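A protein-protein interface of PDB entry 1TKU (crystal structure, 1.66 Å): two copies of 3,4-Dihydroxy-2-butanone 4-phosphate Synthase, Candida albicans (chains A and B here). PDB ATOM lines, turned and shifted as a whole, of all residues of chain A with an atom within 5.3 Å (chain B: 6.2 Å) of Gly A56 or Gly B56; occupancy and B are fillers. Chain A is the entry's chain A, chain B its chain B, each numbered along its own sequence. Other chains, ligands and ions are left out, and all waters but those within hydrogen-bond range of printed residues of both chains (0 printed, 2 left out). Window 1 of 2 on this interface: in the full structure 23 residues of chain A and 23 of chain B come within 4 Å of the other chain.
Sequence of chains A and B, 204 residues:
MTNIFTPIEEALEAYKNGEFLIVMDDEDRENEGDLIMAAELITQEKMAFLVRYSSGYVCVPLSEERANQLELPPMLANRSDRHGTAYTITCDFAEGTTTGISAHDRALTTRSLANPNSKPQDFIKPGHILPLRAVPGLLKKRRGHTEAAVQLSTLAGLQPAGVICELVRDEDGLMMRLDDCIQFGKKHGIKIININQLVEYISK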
ATOM      1  N   VAL A  51     -33.868   1.344  28.994  1.00  0.00           N
ATOM      2  CA  VAL A  51     -32.415   1.235  29.037  1.00  0.00           C
ATOM      3  C   VAL A  51     -31.976  -0.078  29.691  1.00  0.00           C
ATOM      4  O   VAL A  51     -31.095  -0.772  29.183  1.00  0.00           O
ATOM      5  CB  VAL A  51     -31.805   2.446  29.797  1.00  0.00           C
ATOM      6  CG1 VAL A  51     -30.324   2.214  30.078  1.00  0.00           C
ATOM      7  CG2 VAL A  51     -31.984   3.708  28.962  1.00  0.00           C
ATOM      8  N   SER A  54     -32.416  -3.030  27.117  1.00  0.00           N
ATOM      9  CA  SER A  54     -32.051  -2.816  25.724  1.00  0.00           C
ATOM     10  C   SER A  54     -30.568  -2.507  25.528  1.00  0.00           C
ATOM     11  O   SER A  54     -29.777  -2.546  26.470  1.00  0.00           O
ATOM     12  CB  SER A  54     -32.871  -1.663  25.150  1.00  0.00           C
ATOM     13  OG  SER A  54     -32.444  -0.431  25.700  1.00  0.00           O
ATOM     14  N   SER A  55     -30.210  -2.188  24.290  1.00  0.00           N
ATOM     15  CA  SER A  55     -28.836  -1.855  23.936  1.00  0.00           C
ATOM     16  C   SER A  55     -28.432  -0.513  24.538  1.00  0.00           C
ATOM     17  O   SER A  55     -27.244  -0.200  24.636  1.00  0.00           O
ATOM     18  CB  SER A  55     -28.695  -1.759  22.420  1.00  0.00           C
ATOM     19  OG  SER A  55     -29.292  -0.558  21.959  1.00  0.00           O
ATOM     20  N   GLY A  56     -29.424   0.289  24.913  1.00  0.00           N
ATOM     21  CA  GLY A  56     -29.133   1.591  25.488  1.00  0.00           C
ATOM     22  C   GLY A  56     -28.937   2.685  24.452  1.00  0.00           C
ATOM     23  O   GLY A  56     -28.870   3.865  24.795  1.00  0.00           O
ATOM     24  N   TYR A  57     -28.834   2.299  23.185  1.00  0.00           N
ATOM     25  CA  TYR A  57     -28.663   3.262  22.098  1.00  0.00           C
ATOM     26  C   TYR A  57     -30.084   3.740  21.782  1.00  0.00           C
ATOM     27  O   TYR A  57     -30.646   3.417  20.736  1.00  0.00           O
ATOM     28  CB  TYR A  57     -28.033   2.554  20.884  1.00  0.00           C
ATOM     29  CG  TYR A  57     -27.186   3.442  19.989  1.00  0.00           C
ATOM     30  CD1 TYR A  57     -26.037   4.066  20.477  1.00  0.00           C
ATOM     31  CD2 TYR A  57     -27.520   3.636  18.650  1.00  0.00           C
ATOM     32  CE1 TYR A  57     -25.241   4.858  19.652  1.00  0.00           C
ATOM     33  CE2 TYR A  57     -26.729   4.426  17.813  1.00  0.00           C
ATOM     34  CZ  TYR A  57     -25.591   5.034  18.320  1.00  0.00           C
ATOM     35  OH  TYR A  57     -24.804   5.815  17.498  1.00  0.00           O
ATOM     36  N   VAL A  58     -30.661   4.511  22.704  1.00  0.00           N
ATOM     37  CA  VAL A  58     -32.036   4.989  22.564  1.00  0.00           C
ATOM     38  C   VAL A  58     -32.243   6.047  21.494  1.00  0.00           C
ATOM     39  O   VAL A  58     -31.625   7.117  21.522  1.00  0.00           O
ATOM     40  CB  VAL A  58     -32.574   5.514  23.916  1.00  0.00           C
ATOM     41  CG1 VAL A  58     -34.016   5.981  23.761  1.00  0.00           C
ATOM     42  CG2 VAL A  58     -32.500   4.406  24.961  1.00  0.00           C
ATOM     43  N   ARG A 106     -32.922  11.786  29.549  1.00  0.00           N
ATOM     44  CA  ARG A 106     -33.258  11.226  28.252  1.00  0.00           C
ATOM     45  C   ARG A 106     -34.770  11.195  28.054  1.00  0.00           C
ATOM     46  O   ARG A 106     -35.257  11.413  26.949  1.00  0.00           O
ATOM     47  CB  ARG A 106     -32.644   9.829  28.079  1.00  0.00           C
ATOM     48  CG  ARG A 106     -31.145   9.898  27.810  1.00  0.00           C
ATOM     49  CD  ARG A 106     -30.627   8.673  27.069  1.00  0.00           C
ATOM     50  NE  ARG A 106     -30.172   7.623  27.976  1.00  0.00           N
ATOM     51  CZ  ARG A 106     -29.612   6.488  27.568  1.00  0.00           C
ATOM     52  NH1 ARG A 106     -29.449   6.264  26.272  1.00  0.00           N
ATOM     53  NH2 ARG A 106     -29.194   5.589  28.452  1.00  0.00           N
ATOM     54  N   CYS A 165     -35.705   1.112  21.114  1.00  0.00           N
ATOM     55  CA  CYS A 165     -34.423   0.498  21.441  1.00  0.00           C
ATOM     56  C   CYS A 165     -34.548  -1.016  21.342  1.00  0.00           C
ATOM     57  O   CYS A 165     -35.620  -1.583  21.585  1.00  0.00           O
ATOM     58  CB  CYS A 165     -33.923   0.910  22.830  1.00  0.00           C
ATOM     59  SG  CYS A 165     -32.092   0.889  22.913  1.00  0.00           S
ATOM     60  N   LEU B  50     -20.348  -4.521  29.494  1.00  0.00           N
ATOM     61  CA  LEU B  50     -20.429  -3.066  29.555  1.00  0.00           C
ATOM     62  C   LEU B  50     -21.850  -2.567  29.290  1.00  0.00           C
ATOM     63  O   LEU B  50     -22.365  -1.731  30.030  1.00  0.00           O
ATOM     64  CB  LEU B  50     -19.455  -2.442  28.544  1.00  0.00           C
ATOM     65  CG  LEU B  50     -19.386  -0.912  28.483  1.00  0.00           C
ATOM     66  CD1 LEU B  50     -18.980  -0.364  29.851  1.00  0.00           C
ATOM     67  CD2 LEU B  50     -18.375  -0.480  27.425  1.00  0.00           C
ATOM     68  N   VAL B  51     -22.485  -3.078  28.240  1.00  0.00           N
ATOM     69  CA  VAL B  51     -23.847  -2.663  27.910  1.00  0.00           C
ATOM     70  C   VAL B  51     -24.835  -3.083  28.998  1.00  0.00           C
ATOM     71  O   VAL B  51     -25.690  -2.302  29.403  1.00  0.00           O
ATOM     72  CB  VAL B  51     -24.296  -3.253  26.544  1.00  0.00           C
ATOM     73  CG1 VAL B  51     -25.785  -3.020  26.327  1.00  0.00           C
ATOM     74  CG2 VAL B  51     -23.505  -2.593  25.420  1.00  0.00           C
ATOM     75  N   SER B  54     -24.552  -0.620  32.047  1.00  0.00           N
ATOM     76  CA  SER B  54     -24.395   0.805  31.777  1.00  0.00           C
ATOM     77  C   SER B  54     -25.573   1.434  31.031  1.00  0.00           C
ATOM     78  O   SER B  54     -26.587   0.789  30.773  1.00  0.00           O
ATOM     79  CB  SER B  54     -23.123   1.027  30.959  1.00  0.00           C
ATOM     80  OG  SER B  54     -23.323   0.624  29.615  1.00  0.00           O
ATOM     81  N   SER B  55     -25.417   2.705  30.681  1.00  0.00           N
ATOM     82  CA  SER B  55     -26.444   3.440  29.953  1.00  0.00           C
ATOM     83  C   SER B  55     -26.569   2.916  28.526  1.00  0.00           C
ATOM     84  O   SER B  55     -27.562   3.174  27.846  1.00  0.00           O
ATOM     85  CB  SER B  55     -26.090   4.926  29.890  1.00  0.00           C
ATOM     86  OG  SER B  55     -25.011   5.130  28.993  1.00  0.00           O
ATOM     87  N   GLY B  56     -25.549   2.200  28.065  1.00  0.00           N
ATOM     88  CA  GLY B  56     -25.587   1.673  26.714  1.00  0.00           C
ATOM     89  C   GLY B  56     -25.133   2.664  25.654  1.00  0.00           C
ATOM     90  O   GLY B  56     -24.988   2.306  24.487  1.00  0.00           O
ATOM     91  N   TYR B  57     -24.920   3.915  26.051  1.00  0.00           N
ATOM     92  CA  TYR B  57     -24.463   4.948  25.120  1.00  0.00           C
ATOM     93  C   TYR B  57     -22.941   4.801  25.120  1.00  0.00           C
ATOM     94  O   TYR B  57     -22.218   5.647  25.653  1.00  0.00           O
ATOM     95  CB  TYR B  57     -24.879   6.333  25.647  1.00  0.00           C
ATOM     96  CG  TYR B  57     -25.093   7.391  24.582  1.00  0.00           C
ATOM     97  CD1 TYR B  57     -26.098   7.252  23.625  1.00  0.00           C
ATOM     98  CD2 TYR B  57     -24.313   8.546  24.551  1.00  0.00           C
ATOM     99  CE1 TYR B  57     -26.323   8.233  22.663  1.00  0.00           C
ATOM    100  CE2 TYR B  57     -24.532   9.541  23.590  1.00  0.00           C
ATOM    101  CZ  TYR B  57     -25.537   9.377  22.651  1.00  0.00           C
ATOM    102  OH  TYR B  57     -25.758  10.348  21.697  1.00  0.00           O
ATOM    103  N   VAL B  58     -22.463   3.713  24.517  1.00  0.00           N
ATOM    104  CA  VAL B  58     -21.034   3.406  24.492  1.00  0.00           C
ATOM    105  C   VAL B  58     -20.200   4.305  23.591  1.00  0.00           C
ATOM    106  O   VAL B  58     -20.458   4.421  22.388  1.00  0.00           O
ATOM    107  CB  VAL B  58     -20.801   1.930  24.104  1.00  0.00           C
ATOM    108  CG1 VAL B  58     -19.316   1.598  24.166  1.00  0.00           C
ATOM    109  CG2 VAL B  58     -21.582   1.024  25.052  1.00  0.00           C
ATOM    110  N   ILE B 101     -25.165  -2.699  16.032  1.00  0.00           N
ATOM    111  CA  ILE B 101     -25.484  -2.486  17.444  1.00  0.00           C
ATOM    112  C   ILE B 101     -25.201  -3.687  18.359  1.00  0.00           C
ATOM    113  O   ILE B 101     -25.105  -3.536  19.578  1.00  0.00           O
ATOM    114  CB  ILE B 101     -26.971  -2.066  17.594  1.00  0.00           C
ATOM    115  CG1 ILE B 101     -27.244  -1.557  19.015  1.00  0.00           C
ATOM    116  CG2 ILE B 101     -27.878  -3.245  17.268  1.00  0.00           C
ATOM    117  CD1 ILE B 101     -26.497  -0.285  19.374  1.00  0.00           C
ATOM    118  N   ARG B 106     -20.290  -3.864  18.004  1.00  0.00           N
ATOM    119  CA  ARG B 106     -19.747  -2.705  18.686  1.00  0.00           C
ATOM    120  C   ARG B 106     -18.333  -2.988  19.183  1.00  0.00           C
ATOM    121  O   ARG B 106     -17.478  -2.110  19.161  1.00  0.00           O
ATOM    122  CB  ARG B 106     -20.670  -2.265  19.831  1.00  0.00           C
ATOM    123  CG  ARG B 106     -21.909  -1.553  19.304  1.00  0.00           C
ATOM    124  CD  ARG B 106     -22.557  -0.649  20.336  1.00  0.00           C
ATOM    125  NE  ARG B 106     -23.562  -1.335  21.140  1.00  0.00           N
ATOM    126  CZ  ARG B 106     -24.284  -0.737  22.082  1.00  0.00           C
ATOM    127  NH1 ARG B 106     -24.099   0.553  22.331  1.00  0.00           N
ATOM    128  NH2 ARG B 106     -25.199  -1.419  22.761  1.00  0.00           N
ATOM    129  N   LEU B 130     -19.969   5.664  19.238  1.00  0.00           N
ATOM    130  CA  LEU B 130     -19.742   7.101  19.385  1.00  0.00           C
ATOM    131  C   LEU B 130     -18.283   7.439  19.709  1.00  0.00           C
ATOM    132  O   LEU B 130     -17.877   7.413  20.868  1.00  0.00           O
ATOM    133  CB  LEU B 130     -20.636   7.653  20.502  1.00  0.00           C
ATOM    134  CG  LEU B 130     -22.155   7.571  20.319  1.00  0.00           C
ATOM    135  CD1 LEU B 130     -22.790   7.007  21.580  1.00  0.00           C
ATOM    136  CD2 LEU B 130     -22.724   8.951  20.014  1.00  0.00           C
ATOM    137  N   CYS B 165     -18.465   3.866  29.365  1.00  0.00           N
ATOM    138  CA  CYS B 165     -19.910   3.992  29.526  1.00  0.00           C
ATOM    139  C   CYS B 165     -20.238   4.131  31.008  1.00  0.00           C
ATOM    140  O   CYS B 165     -19.519   3.609  31.864  1.00  0.00           O
ATOM    141  CB  CYS B 165     -20.657   2.799  28.927  1.00  0.00           C
ATOM    142  SG  CYS B 165     -22.332   3.267  28.365  1.00  0.00           S
ATOM    143  N   GLU B 166     -21.325   4.841  31.297  1.00  0.00           N
ATOM    144  CA  GLU B 166     -21.767   5.104  32.668  1.00  0.00           C
ATOM    145  C   GLU B 166     -22.491   3.946  33.351  1.00  0.00           C
ATOM    146  O   GLU B 166     -23.445   3.395  32.802  1.00  0.00           O
ATOM    147  CB  GLU B 166     -22.704   6.320  32.690  1.00  0.00           C
ATOM    148  CG  GLU B 166     -22.183   7.575  32.006  1.00  0.00           C
ATOM    149  CD  GLU B 166     -22.574   7.674  30.537  1.00  0.00           C
ATOM    150  OE1 GLU B 166     -22.454   8.783  29.977  1.00  0.00           O
ATOM    151  OE2 GLU B 166     -22.993   6.661  29.936  1.00  0.00           O
ATOM    152  N   VAL B 168     -25.054   2.064  35.672  1.00  0.00           N
ATOM    153  CA  VAL B 168     -26.422   2.383  36.082  1.00  0.00           C
ATOM    154  C   VAL B 168     -26.980   1.288  36.981  1.00  0.00           C
ATOM    155  O   VAL B 168     -26.702   0.103  36.780  1.00  0.00           O
ATOM    156  CB  VAL B 168     -27.371   2.546  34.866  1.00  0.00           C
ATOM    157  CG1 VAL B 168     -26.842   3.615  33.926  1.00  0.00           C
ATOM    158  CG2 VAL B 168     -27.519   1.226  34.139  1.00  0.00           C
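The backbone carbonyl oxygen of Ser A55 sits at hydrogen-bond distance from the guanidinium group of Arg B106 (3.0 Å).
NH2 of Arg A106 is in hydrogen-bond range of O of Ser B55 (3.0 Å).
The backbone carbonyl oxygen (O) of Gly B56 sits close to the backbone carbonyl oxygen (O) of Ser A55 (3.4 Å).
The backbone carbonyl oxygen of Ser B55 sits close to the backbone carbonyl oxygen of Gly A56, 3.4 Å away.
The backbone carbonyl oxygen (O) of Gly A56 is in hydrogen-bond range of the guanidinium group (NH1) of Arg A106.
N of Gly B56 sits close to OG of Ser B54, 3.1 Å away.
The side-chain hydroxyl of Ser B55 lies within hydrogen-bond range of the side-chain sulfur of Cys B165 (3.3 Å).
OG of Ser B55 is in hydrogen-bond range of OE2 of Glu B166.
N of Gly B56 lies within hydrogen-bond range of SG of Cys B165 (3.4 Å).
The guanidinium group (NE) of Arg B106 lies within hydrogen-bond range of the backbone carbonyl oxygen (O) of Ile B101 (3.1 Å).
CG1 of Val A51 touches O of Ser B55, at 3.7 Å.
Ser A55 touches Val B51 (O to CG1, 3.6 Å).
CG1 of Ile B101 touches CB of Ser A55, at 3.7 Å.
Gly A56 touches Gly B56 (CA to CA, 3.8 Å).
Tyr A57 touches Ile B101.
Leu B130 touches Tyr A57.
Gly A56 touches two residues of chain B.
Gly B56 touches just these residues of chain A: Ser A55 (3.3 Å) and Gly A56 (3.8 Å).
Of the printed residues of chain B, Tyr A57 touches Ile B101 (3.6 Å) and Leu B130 (3.8 Å).
Of the printed residues of chain A, Leu B130 touches Tyr A57.
Of the printed residues of chain A, Arg B106 touches Ser A55 (3.0 Å).
Of the printed residues of chain A, Ser B55 touches Val A51, Gly A56 and Arg A106.
The nearest residue of chain A that does not touch Gly B56 is Tyr A57 (4.1 Å).
Hydrophobic or aromatic side chains of chain B within 4 Å of the printed part of chain A: Val B51, Ile B101 and Leu B130.
Along chain B the printed residues that touch a printed residue of chain A span positions 51 to 130.
Printed residues of chain A that touch a printed residue of chain B: Val A51, Ser A55, Gly A56, Tyr A57 and Arg A106.
Among the printed residues, 10 pairs touch across the chains.
Among the printed residues, no Asp or Glu carboxylate lies within 4 Å of a Lys or Arg side-chain nitrogen of the other chain.
Val A51 touches Ser B55, and with the chains exchanged Ser A55 touches Val B51.
Ser A55 touches Gly B56, and with the chains exchanged Gly A56 touches Ser B55.
Ser A55 touches Arg B106, and with the chains exchanged Arg A106 touches Ser B55.
Gly A56 touches its own counterpart, Gly B56.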
